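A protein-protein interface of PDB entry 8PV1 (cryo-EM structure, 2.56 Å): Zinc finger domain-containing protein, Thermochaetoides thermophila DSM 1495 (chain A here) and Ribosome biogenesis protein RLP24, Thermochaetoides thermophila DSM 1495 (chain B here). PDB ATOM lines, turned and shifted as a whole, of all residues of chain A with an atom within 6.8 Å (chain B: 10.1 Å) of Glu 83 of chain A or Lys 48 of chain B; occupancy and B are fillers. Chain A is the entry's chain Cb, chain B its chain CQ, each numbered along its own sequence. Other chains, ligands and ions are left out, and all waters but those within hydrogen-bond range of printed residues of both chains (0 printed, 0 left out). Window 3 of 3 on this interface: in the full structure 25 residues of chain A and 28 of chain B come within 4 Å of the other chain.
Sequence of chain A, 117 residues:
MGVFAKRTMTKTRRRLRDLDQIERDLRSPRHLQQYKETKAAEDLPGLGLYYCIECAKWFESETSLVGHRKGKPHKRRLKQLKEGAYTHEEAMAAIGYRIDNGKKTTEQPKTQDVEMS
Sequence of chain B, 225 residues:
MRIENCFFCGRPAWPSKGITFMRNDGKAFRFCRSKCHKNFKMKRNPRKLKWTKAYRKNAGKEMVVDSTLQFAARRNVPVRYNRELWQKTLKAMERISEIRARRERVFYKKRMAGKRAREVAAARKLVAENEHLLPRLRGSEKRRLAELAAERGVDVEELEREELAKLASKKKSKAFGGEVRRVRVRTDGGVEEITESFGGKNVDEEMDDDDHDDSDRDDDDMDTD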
ATOM      1  N   GLU A  23      -7.392  -7.241 -16.339  1.00  0.00           N
ATOM      2  CA  GLU A  23      -7.670  -6.312 -15.239  1.00  0.00           C
ATOM      3  C   GLU A  23      -7.704  -7.030 -13.901  1.00  0.00           C
ATOM      4  O   GLU A  23      -7.263  -6.483 -12.886  1.00  0.00           O
ATOM      5  CB  GLU A  23      -8.986  -5.546 -15.393  1.00  0.00           C
ATOM      6  CG  GLU A  23      -9.443  -5.067 -16.726  1.00  0.00           C
ATOM      7  CD  GLU A  23     -10.611  -4.123 -16.544  1.00  0.00           C
ATOM      8  OE1 GLU A  23     -10.583  -3.347 -15.570  1.00  0.00           O
ATOM      9  OE2 GLU A  23     -11.566  -4.157 -17.334  1.00  0.00           O
ATOM     10  N   ARG A  76      -1.915   0.300 -27.089  1.00  0.00           N
ATOM     11  CA  ARG A  76      -3.316  -0.044 -27.320  1.00  0.00           C
ATOM     12  C   ARG A  76      -3.894  -0.798 -26.133  1.00  0.00           C
ATOM     13  O   ARG A  76      -5.026  -0.529 -25.711  1.00  0.00           O
ATOM     14  CB  ARG A  76      -3.484  -0.868 -28.599  1.00  0.00           C
ATOM     15  CG  ARG A  76      -4.930  -1.335 -28.785  1.00  0.00           C
ATOM     16  CD  ARG A  76      -5.312  -1.777 -30.179  1.00  0.00           C
ATOM     17  NE  ARG A  76      -4.669  -3.015 -30.590  1.00  0.00           N
ATOM     18  CZ  ARG A  76      -4.995  -3.695 -31.681  1.00  0.00           C
ATOM     19  NH1 ARG A  76      -5.989  -3.310 -32.464  1.00  0.00           N
ATOM     20  NH2 ARG A  76      -4.312  -4.793 -31.988  1.00  0.00           N
ATOM     21  N   LEU A  78      -2.845  -0.529 -23.056  1.00  0.00           N
ATOM     22  CA  LEU A  78      -2.962   0.454 -21.982  1.00  0.00           C
ATOM     23  C   LEU A  78      -4.212   1.314 -22.135  1.00  0.00           C
ATOM     24  O   LEU A  78      -4.921   1.568 -21.155  1.00  0.00           O
ATOM     25  CB  LEU A  78      -1.713   1.332 -21.934  1.00  0.00           C
ATOM     26  CG  LEU A  78      -0.463   0.690 -21.336  1.00  0.00           C
ATOM     27  CD1 LEU A  78       0.750   1.562 -21.593  1.00  0.00           C
ATOM     28  CD2 LEU A  78      -0.647   0.445 -19.850  1.00  0.00           C
ATOM     29  N   LYS A  79      -4.510   1.759 -23.359  1.00  0.00           N
ATOM     30  CA  LYS A  79      -5.695   2.587 -23.559  1.00  0.00           C
ATOM     31  C   LYS A  79      -6.974   1.770 -23.404  1.00  0.00           C
ATOM     32  O   LYS A  79      -7.991   2.279 -22.916  1.00  0.00           O
ATOM     33  CB  LYS A  79      -5.642   3.269 -24.926  1.00  0.00           C
ATOM     34  CG  LYS A  79      -6.787   4.241 -25.164  1.00  0.00           C
ATOM     35  CD  LYS A  79      -6.666   4.967 -26.489  1.00  0.00           C
ATOM     36  CE  LYS A  79      -7.834   5.923 -26.685  1.00  0.00           C
ATOM     37  NZ  LYS A  79      -7.754   6.655 -27.974  1.00  0.00           N
ATOM     38  N   GLN A  80      -6.936   0.491 -23.786  1.00  0.00           N
ATOM     39  CA  GLN A  80      -8.094  -0.375 -23.586  1.00  0.00           C
ATOM     40  C   GLN A  80      -8.345  -0.629 -22.106  1.00  0.00           C
ATOM     41  O   GLN A  80      -9.498  -0.668 -21.665  1.00  0.00           O
ATOM     42  CB  GLN A  80      -7.900  -1.694 -24.330  1.00  0.00           C
ATOM     43  CG  GLN A  80      -8.208  -1.637 -25.811  1.00  0.00           C
ATOM     44  CD  GLN A  80      -7.840  -2.920 -26.521  1.00  0.00           C
ATOM     45  OE1 GLN A  80      -7.165  -3.778 -25.959  1.00  0.00           O
ATOM     46  NE2 GLN A  80      -8.281  -3.058 -27.762  1.00  0.00           N
ATOM     47  N   LEU A  81      -7.277  -0.798 -21.324  1.00  0.00           N
ATOM     48  CA  LEU A  81      -7.431  -0.950 -19.882  1.00  0.00           C
ATOM     49  C   LEU A  81      -7.895   0.347 -19.231  1.00  0.00           C
ATOM     50  O   LEU A  81      -8.625   0.317 -18.234  1.00  0.00           O
ATOM     51  CB  LEU A  81      -6.120  -1.425 -19.265  1.00  0.00           C
ATOM     52  CG  LEU A  81      -5.773  -2.882 -19.553  1.00  0.00           C
ATOM     53  CD1 LEU A  81      -4.327  -3.147 -19.242  1.00  0.00           C
ATOM     54  CD2 LEU A  81      -6.660  -3.797 -18.742  1.00  0.00           C
ATOM     55  N   LYS A  82      -7.468   1.493 -19.765  1.00  0.00           N
ATOM     56  CA  LYS A  82      -7.953   2.772 -19.255  1.00  0.00           C
ATOM     57  C   LYS A  82      -9.441   2.945 -19.536  1.00  0.00           C
ATOM     58  O   LYS A  82     -10.185   3.452 -18.688  1.00  0.00           O
ATOM     59  CB  LYS A  82      -7.148   3.918 -19.864  1.00  0.00           C
ATOM     60  CG  LYS A  82      -7.548   5.294 -19.365  1.00  0.00           C
ATOM     61  CD  LYS A  82      -6.624   6.370 -19.906  1.00  0.00           C
ATOM     62  CE  LYS A  82      -6.882   6.630 -21.380  1.00  0.00           C
ATOM     63  NZ  LYS A  82      -6.063   7.763 -21.890  1.00  0.00           N
ATOM     64  N   GLU A  83      -9.894   2.524 -20.719  1.00  0.00           N
ATOM     65  CA  GLU A  83     -11.322   2.553 -21.022  1.00  0.00           C
ATOM     66  C   GLU A  83     -12.100   1.550 -20.177  1.00  0.00           C
ATOM     67  O   GLU A  83     -13.251   1.813 -19.814  1.00  0.00           O
ATOM     68  CB  GLU A  83     -11.556   2.278 -22.507  1.00  0.00           C
ATOM     69  CG  GLU A  83     -11.260   3.456 -23.412  1.00  0.00           C
ATOM     70  CD  GLU A  83     -11.402   3.109 -24.877  1.00  0.00           C
ATOM     71  OE1 GLU A  83     -11.195   1.931 -25.236  1.00  0.00           O
ATOM     72  OE2 GLU A  83     -11.734   4.014 -25.672  1.00  0.00           O
ATOM     73  N   GLY A  84     -11.495   0.408 -19.857  1.00  0.00           N
ATOM     74  CA  GLY A  84     -12.155  -0.622 -19.081  1.00  0.00           C
ATOM     75  C   GLY A  84     -12.736  -1.711 -19.958  1.00  0.00           C
ATOM     76  O   GLY A  84     -13.383  -1.412 -20.965  1.00  0.00           O
ATOM     77  N   ALA A  85     -12.516  -2.973 -19.601  1.00  0.00           N
ATOM     78  CA  ALA A  85     -13.050  -4.060 -20.407  1.00  0.00           C
ATOM     79  C   ALA A  85     -14.524  -4.291 -20.103  1.00  0.00           C
ATOM     80  O   ALA A  85     -15.068  -3.798 -19.111  1.00  0.00           O
ATOM     81  CB  ALA A  85     -12.269  -5.354 -20.185  1.00  0.00           C
ATOM     82  N   GLU A  90     -21.456  -4.706 -16.604  1.00  0.00           N
ATOM     83  CA  GLU A  90     -21.742  -3.711 -17.630  1.00  0.00           C
ATOM     84  C   GLU A  90     -22.826  -4.202 -18.580  1.00  0.00           C
ATOM     85  O   GLU A  90     -23.657  -3.411 -19.042  1.00  0.00           O
ATOM     86  CB  GLU A  90     -20.460  -3.365 -18.388  1.00  0.00           C
ATOM     87  CG  GLU A  90     -20.634  -2.339 -19.492  1.00  0.00           C
ATOM     88  CD  GLU A  90     -19.313  -1.821 -20.016  1.00  0.00           C
ATOM     89  OE1 GLU A  90     -18.261  -2.232 -19.485  1.00  0.00           O
ATOM     90  OE2 GLU A  90     -19.323  -1.009 -20.963  1.00  0.00           O
ATOM     91  N   PHE B   8     -23.110  -9.988 -25.539  1.00  0.00           N
ATOM     92  CA  PHE B   8     -22.465  -9.008 -26.400  1.00  0.00           C
ATOM     93  C   PHE B   8     -23.400  -7.859 -26.762  1.00  0.00           C
ATOM     94  O   PHE B   8     -23.030  -6.688 -26.633  1.00  0.00           O
ATOM     95  CB  PHE B   8     -21.951  -9.700 -27.660  1.00  0.00           C
ATOM     96  CG  PHE B   8     -20.840  -8.972 -28.342  1.00  0.00           C
ATOM     97  CD1 PHE B   8     -21.113  -8.003 -29.291  1.00  0.00           C
ATOM     98  CD2 PHE B   8     -19.521  -9.260 -28.044  1.00  0.00           C
ATOM     99  CE1 PHE B   8     -20.092  -7.331 -29.920  1.00  0.00           C
ATOM    100  CE2 PHE B   8     -18.494  -8.594 -28.675  1.00  0.00           C
ATOM    101  CZ  PHE B   8     -18.780  -7.625 -29.610  1.00  0.00           C
ATOM    102  N   ASN B  39     -17.744 -11.763 -33.167  1.00  0.00           N
ATOM    103  CA  ASN B  39     -17.173 -10.497 -32.712  1.00  0.00           C
ATOM    104  C   ASN B  39     -16.485 -10.657 -31.357  1.00  0.00           C
ATOM    105  O   ASN B  39     -15.420 -10.069 -31.115  1.00  0.00           O
ATOM    106  CB  ASN B  39     -18.259  -9.423 -32.666  1.00  0.00           C
ATOM    107  CG  ASN B  39     -18.484  -8.772 -34.018  1.00  0.00           C
ATOM    108  OD1 ASN B  39     -17.559  -8.231 -34.616  1.00  0.00           O
ATOM    109  ND2 ASN B  39     -19.713  -8.838 -34.513  1.00  0.00           N
ATOM    110  N   LYS B  43     -12.528 -10.317 -30.323  1.00  0.00           N
ATOM    111  CA  LYS B  43     -12.218  -9.420 -29.200  1.00  0.00           C
ATOM    112  C   LYS B  43     -12.596  -7.977 -29.524  1.00  0.00           C
ATOM    113  O   LYS B  43     -11.886  -7.038 -29.160  1.00  0.00           O
ATOM    114  CB  LYS B  43     -10.748  -9.497 -28.756  1.00  0.00           C
ATOM    115  CG  LYS B  43     -10.135 -10.887 -28.667  1.00  0.00           C
ATOM    116  CD  LYS B  43     -10.616 -11.648 -27.451  1.00  0.00           C
ATOM    117  CE  LYS B  43      -9.822 -12.930 -27.279  1.00  0.00           C
ATOM    118  NZ  LYS B  43     -10.193 -13.658 -26.039  1.00  0.00           N
ATOM    119  N   ARG B  44     -13.714  -7.800 -30.216  1.00  0.00           N
ATOM    120  CA  ARG B  44     -14.265  -6.473 -30.434  1.00  0.00           C
ATOM    121  C   ARG B  44     -15.041  -6.032 -29.201  1.00  0.00           C
ATOM    122  O   ARG B  44     -15.783  -6.816 -28.607  1.00  0.00           O
ATOM    123  CB  ARG B  44     -15.167  -6.468 -31.665  1.00  0.00           C
ATOM    124  CG  ARG B  44     -14.485  -6.958 -32.928  1.00  0.00           C
ATOM    125  CD  ARG B  44     -14.916  -6.149 -34.133  1.00  0.00           C
ATOM    126  NE  ARG B  44     -14.351  -4.807 -34.131  1.00  0.00           N
ATOM    127  CZ  ARG B  44     -14.649  -3.872 -35.023  1.00  0.00           C
ATOM    128  NH1 ARG B  44     -15.507  -4.101 -36.002  1.00  0.00           N
ATOM    129  NH2 ARG B  44     -14.074  -2.678 -34.927  1.00  0.00           N
ATOM    130  N   ASN B  45     -14.855  -4.775 -28.809  1.00  0.00           N
ATOM    131  CA  ASN B  45     -15.528  -4.236 -27.635  1.00  0.00           C
ATOM    132  C   ASN B  45     -16.985  -3.949 -27.971  1.00  0.00           C
ATOM    133  O   ASN B  45     -17.251  -3.229 -28.942  1.00  0.00           O
ATOM    134  CB  ASN B  45     -14.842  -2.963 -27.165  1.00  0.00           C
ATOM    135  CG  ASN B  45     -15.113  -2.650 -25.704  1.00  0.00           C
ATOM    136  OD1 ASN B  45     -16.005  -3.221 -25.084  1.00  0.00           O
ATOM    137  ND2 ASN B  45     -14.332  -1.736 -25.148  1.00  0.00           N
ATOM    138  N   PRO B  46     -17.950  -4.505 -27.229  1.00  0.00           N
ATOM    139  CA  PRO B  46     -19.361  -4.157 -27.479  1.00  0.00           C
ATOM    140  C   PRO B  46     -19.681  -2.693 -27.245  1.00  0.00           C
ATOM    141  O   PRO B  46     -20.631  -2.167 -27.838  1.00  0.00           O
ATOM    142  CB  PRO B  46     -20.119  -5.057 -26.495  1.00  0.00           C
ATOM    143  CG  PRO B  46     -19.210  -6.176 -26.226  1.00  0.00           C
ATOM    144  CD  PRO B  46     -17.819  -5.634 -26.295  1.00  0.00           C
ATOM    145  N   ARG B  47     -18.913  -2.024 -26.384  1.00  0.00           N
ATOM    146  CA  ARG B  47     -19.146  -0.617 -26.086  1.00  0.00           C
ATOM    147  C   ARG B  47     -18.816   0.289 -27.266  1.00  0.00           C
ATOM    148  O   ARG B  47     -19.271   1.437 -27.300  1.00  0.00           O
ATOM    149  CB  ARG B  47     -18.321  -0.220 -24.860  1.00  0.00           C
ATOM    150  CG  ARG B  47     -18.840   0.980 -24.099  1.00  0.00           C
ATOM    151  CD  ARG B  47     -17.848   1.428 -23.040  1.00  0.00           C
ATOM    152  NE  ARG B  47     -17.544   0.371 -22.085  1.00  0.00           N
ATOM    153  CZ  ARG B  47     -16.335  -0.133 -21.881  1.00  0.00           C
ATOM    154  NH1 ARG B  47     -15.282   0.304 -22.552  1.00  0.00           N
ATOM    155  NH2 ARG B  47     -16.178  -1.094 -20.977  1.00  0.00           N
ATOM    156  N   LYS B  48     -18.045  -0.202 -28.238  1.00  0.00           N
ATOM    157  CA  LYS B  48     -17.687   0.580 -29.412  1.00  0.00           C
ATOM    158  C   LYS B  48     -18.517   0.250 -30.644  1.00  0.00           C
ATOM    159  O   LYS B  48     -18.556   1.061 -31.575  1.00  0.00           O
ATOM    160  CB  LYS B  48     -16.205   0.382 -29.746  1.00  0.00           C
ATOM    161  CG  LYS B  48     -15.265   1.042 -28.759  1.00  0.00           C
ATOM    162  CD  LYS B  48     -13.822   0.885 -29.188  1.00  0.00           C
ATOM    163  CE  LYS B  48     -12.892   1.605 -28.235  1.00  0.00           C
ATOM    164  NZ  LYS B  48     -13.080   3.079 -28.310  1.00  0.00           N
ATOM    165  N   LEU B  49     -19.174  -0.906 -30.679  1.00  0.00           N
ATOM    166  CA  LEU B  49     -20.009  -1.273 -31.816  1.00  0.00           C
ATOM    167  C   LEU B  49     -21.385  -0.645 -31.648  1.00  0.00           C
ATOM    168  O   LEU B  49     -22.112  -0.978 -30.707  1.00  0.00           O
ATOM    169  CB  LEU B  49     -20.113  -2.791 -31.939  1.00  0.00           C
ATOM    170  CG  LEU B  49     -18.800  -3.547 -32.142  1.00  0.00           C
ATOM    171  CD1 LEU B  49     -19.067  -5.004 -32.453  1.00  0.00           C
ATOM    172  CD2 LEU B  49     -17.973  -2.913 -33.243  1.00  0.00           C
ATOM    173  N   LYS B  50     -21.753   0.237 -32.580  1.00  0.00           N
ATOM    174  CA  LYS B  50     -22.908   1.109 -32.390  1.00  0.00           C
ATOM    175  C   LYS B  50     -24.238   0.369 -32.436  1.00  0.00           C
ATOM    176  O   LYS B  50     -25.263   0.941 -32.053  1.00  0.00           O
ATOM    177  CB  LYS B  50     -22.894   2.224 -33.433  1.00  0.00           C
ATOM    178  CG  LYS B  50     -21.644   3.075 -33.387  1.00  0.00           C
ATOM    179  CD  LYS B  50     -21.643   4.135 -34.469  1.00  0.00           C
ATOM    180  CE  LYS B  50     -20.324   4.882 -34.492  1.00  0.00           C
ATOM    181  NZ  LYS B  50     -20.160   5.732 -33.284  1.00  0.00           N
ATOM    182  N   TRP B  51     -24.251  -0.882 -32.880  1.00  0.00           N
ATOM    183  CA  TRP B  51     -25.478  -1.658 -32.933  1.00  0.00           C
ATOM    184  C   TRP B  51     -25.778  -2.400 -31.636  1.00  0.00           C
ATOM    185  O   TRP B  51     -26.650  -3.273 -31.635  1.00  0.00           O
ATOM    186  CB  TRP B  51     -25.419  -2.642 -34.106  1.00  0.00           C
ATOM    187  CG  TRP B  51     -24.192  -3.508 -34.132  1.00  0.00           C
ATOM    188  CD1 TRP B  51     -22.990  -3.208 -34.699  1.00  0.00           C
ATOM    189  CD2 TRP B  51     -24.055  -4.817 -33.574  1.00  0.00           C
ATOM    190  NE1 TRP B  51     -22.111  -4.244 -34.525  1.00  0.00           N
ATOM    191  CE2 TRP B  51     -22.741  -5.247 -33.840  1.00  0.00           C
ATOM    192  CE3 TRP B  51     -24.916  -5.669 -32.878  1.00  0.00           C
ATOM    193  CZ2 TRP B  51     -22.266  -6.490 -33.429  1.00  0.00           C
ATOM    194  CZ3 TRP B  51     -24.446  -6.897 -32.475  1.00  0.00           C
ATOM    195  CH2 TRP B  51     -23.132  -7.299 -32.750  1.00  0.00           C
ATOM    196  N   THR B  52     -25.100  -2.080 -30.538  1.00  0.00           N
ATOM    197  CA  THR B  52     -25.306  -2.803 -29.292  1.00  0.00           C
ATOM    198  C   THR B  52     -25.905  -1.913 -28.203  1.00  0.00           C
ATOM    199  O   THR B  52     -25.736  -0.686 -28.183  1.00  0.00           O
ATOM    200  CB  THR B  52     -23.996  -3.412 -28.786  1.00  0.00           C
ATOM    201  OG1 THR B  52     -23.105  -2.371 -28.371  1.00  0.00           O
ATOM    202  CG2 THR B  52     -23.333  -4.253 -29.868  1.00  0.00           C
ATOM    203  N   LYS B  53     -26.602  -2.571 -27.271  1.00  0.00           N
ATOM    204  CA  LYS B  53     -27.117  -1.891 -26.089  1.00  0.00           C
ATOM    205  C   LYS B  53     -25.999  -1.356 -25.207  1.00  0.00           C
ATOM    206  O   LYS B  53     -26.203  -0.372 -24.495  1.00  0.00           O
ATOM    207  CB  LYS B  53     -28.012  -2.832 -25.282  1.00  0.00           C
ATOM    208  CG  LYS B  53     -29.321  -3.191 -25.952  1.00  0.00           C
ATOM    209  CD  LYS B  53     -30.228  -1.974 -26.037  1.00  0.00           C
ATOM    210  CE  LYS B  53     -31.594  -2.340 -26.573  1.00  0.00           C
ATOM    211  NZ  LYS B  53     -32.497  -1.172 -26.728  1.00  0.00           N
ATOM    212  N   ALA B  54     -24.821  -1.980 -25.247  1.00  0.00           N
ATOM    213  CA  ALA B  54     -23.677  -1.467 -24.501  1.00  0.00           C
ATOM    214  C   ALA B  54     -23.264  -0.090 -25.006  1.00  0.00           C
ATOM    215  O   ALA B  54     -23.079   0.844 -24.213  1.00  0.00           O
ATOM    216  CB  ALA B  54     -22.512  -2.444 -24.600  1.00  0.00           C
ATOM    217  N   TYR B  55     -23.142   0.058 -26.329  1.00  0.00           N
ATOM    218  CA  TYR B  55     -22.834   1.362 -26.906  1.00  0.00           C
ATOM    219  C   TYR B  55     -23.945   2.354 -26.618  1.00  0.00           C
ATOM    220  O   TYR B  55     -23.682   3.527 -26.339  1.00  0.00           O
ATOM    221  CB  TYR B  55     -22.608   1.253 -28.418  1.00  0.00           C
ATOM    222  CG  TYR B  55     -22.558   2.594 -29.153  1.00  0.00           C
ATOM    223  CD1 TYR B  55     -21.356   3.263 -29.319  1.00  0.00           C
ATOM    224  CD2 TYR B  55     -23.707   3.175 -29.696  1.00  0.00           C
ATOM    225  CE1 TYR B  55     -21.299   4.474 -29.981  1.00  0.00           C
ATOM    226  CE2 TYR B  55     -23.656   4.380 -30.351  1.00  0.00           C
ATOM    227  CZ  TYR B  55     -22.452   5.026 -30.492  1.00  0.00           C
ATOM    228  OH  TYR B  55     -22.406   6.228 -31.157  1.00  0.00           O
ATOM    229  N   ARG B  56     -25.199   1.914 -26.742  1.00  0.00           N
ATOM    230  CA  ARG B  56     -26.310   2.844 -26.576  1.00  0.00           C
ATOM    231  C   ARG B  56     -26.406   3.349 -25.136  1.00  0.00           C
ATOM    232  O   ARG B  56     -26.676   4.533 -24.902  1.00  0.00           O
ATOM    233  CB  ARG B  56     -27.606   2.179 -27.027  1.00  0.00           C
ATOM    234  CG  ARG B  56     -27.686   1.977 -28.532  1.00  0.00           C
ATOM    235  CD  ARG B  56     -28.938   1.213 -28.929  1.00  0.00           C
ATOM    236  NE  ARG B  56     -30.161   1.987 -28.744  1.00  0.00           N
ATOM    237  CZ  ARG B  56     -30.521   3.041 -29.467  1.00  0.00           C
ATOM    238  NH1 ARG B  56     -29.815   3.444 -30.512  1.00  0.00           N
ATOM    239  NH2 ARG B  56     -31.633   3.694 -29.149  1.00  0.00           N
ATOM    240  N   LYS B  57     -26.150   2.473 -24.161  1.00  0.00           N
ATOM    241  CA  LYS B  57     -26.135   2.893 -22.766  1.00  0.00           C
ATOM    242  C   LYS B  57     -24.924   3.767 -22.463  1.00  0.00           C
ATOM    243  O   LYS B  57     -25.012   4.691 -21.647  1.00  0.00           O
ATOM    244  CB  LYS B  57     -26.158   1.667 -21.852  1.00  0.00           C
ATOM    245  CG  LYS B  57     -26.600   1.946 -20.422  1.00  0.00           C
ATOM    246  CD  LYS B  57     -25.420   2.107 -19.478  1.00  0.00           C
ATOM    247  CE  LYS B  57     -25.886   2.398 -18.065  1.00  0.00           C
ATOM    248  NZ  LYS B  57     -24.739   2.583 -17.136  1.00  0.00           N
ATOM    249  N   ASN B  58     -23.780   3.483 -23.095  1.00  0.00           N
ATOM    250  CA  ASN B  58     -22.606   4.327 -22.899  1.00  0.00           C
ATOM    251  C   ASN B  58     -22.801   5.711 -23.503  1.00  0.00           C
ATOM    252  O   ASN B  58     -22.301   6.702 -22.961  1.00  0.00           O
ATOM    253  CB  ASN B  58     -21.375   3.653 -23.501  1.00  0.00           C
ATOM    254  CG  ASN B  58     -20.087   4.328 -23.093  1.00  0.00           C
ATOM    255  OD1 ASN B  58     -19.827   4.529 -21.909  1.00  0.00           O
ATOM    256  ND2 ASN B  58     -19.268   4.681 -24.075  1.00  0.00           N
ATOM    257  N   ALA B  59     -23.515   5.797 -24.621  1.00  0.00           N
ATOM    258  CA  ALA B  59     -23.775   7.063 -25.290  1.00  0.00           C
ATOM    259  C   ALA B  59     -25.001   7.779 -24.744  1.00  0.00           C
ATOM    260  O   ALA B  59     -25.250   8.924 -25.131  1.00  0.00           O
ATOM    261  CB  ALA B  59     -23.939   6.835 -26.795  1.00  0.00           C
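The guanidinium group (NE) of Arg 47 of chain B is in salt-bridge range of the side-chain carboxylate (OE2) of Glu 90 of chain A, 2.5 Å away.
The backbone carbonyl oxygen of Gly 84 of chain A sits at hydrogen-bond distance from the guanidinium group of Arg 47 of chain B (2.8 Å).
NH2 of Arg 47 of chain B sits at hydrogen-bond distance from O of Ala 85 of chain A (3.5 Å).
OE2 of Glu 83 of chain A lies within salt-bridge range of NZ of Lys 48 of chain B, 3.1 Å away.
Of chain A, only Glu 83 (3.1 Å) comes within 4 Å of Lys 48 of chain B.
Of chain B, only Arg 47 (2.8 Å) comes within 4 Å of Gly 84 of chain A.
Of the printed residues of chain B, Glu 90 of chain A touches Arg 47.
Printed residues of chain A within 4 Å of Arg 47 of chain B: Glu 83, Gly 84, Ala 85 and Glu 90.
Printed residues of chain B within 4 Å of Ala 85 of chain A: Arg 47 (3.5 Å).
Lys 53 of chain B touches none of the printed residues of chain A.
The nearest residue of chain B that does not touch Glu 83 of chain A is Asn 45 of chain B (4.8 Å).
The nearest printed residue of chain A that does not touch Lys 48 of chain B is Lys 79 of chain A (6.2 Å).
The backbone NH (N) of Ala 85 of chain A is in hydrogen-bond range of the side-chain carboxylate (OE2) of Glu 23 of chain A (2.7 Å).
The side-chain amide oxygen (OD1) of Asn 45 of chain B sits close to the backbone NH (N) of Arg 47 of chain B (3.4 Å).
Among the printed residues, pairs that only touch across the chains: Glu 83 of chain A with Arg 47 of chain B.
Of the 11 printed residues of chain A, 4 touch a printed residue of chain B.
Printed residues of chain B that touch a printed residue of chain A: Arg 47 and Lys 48.
Among the printed residues, 5 pairs touch across the chains.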
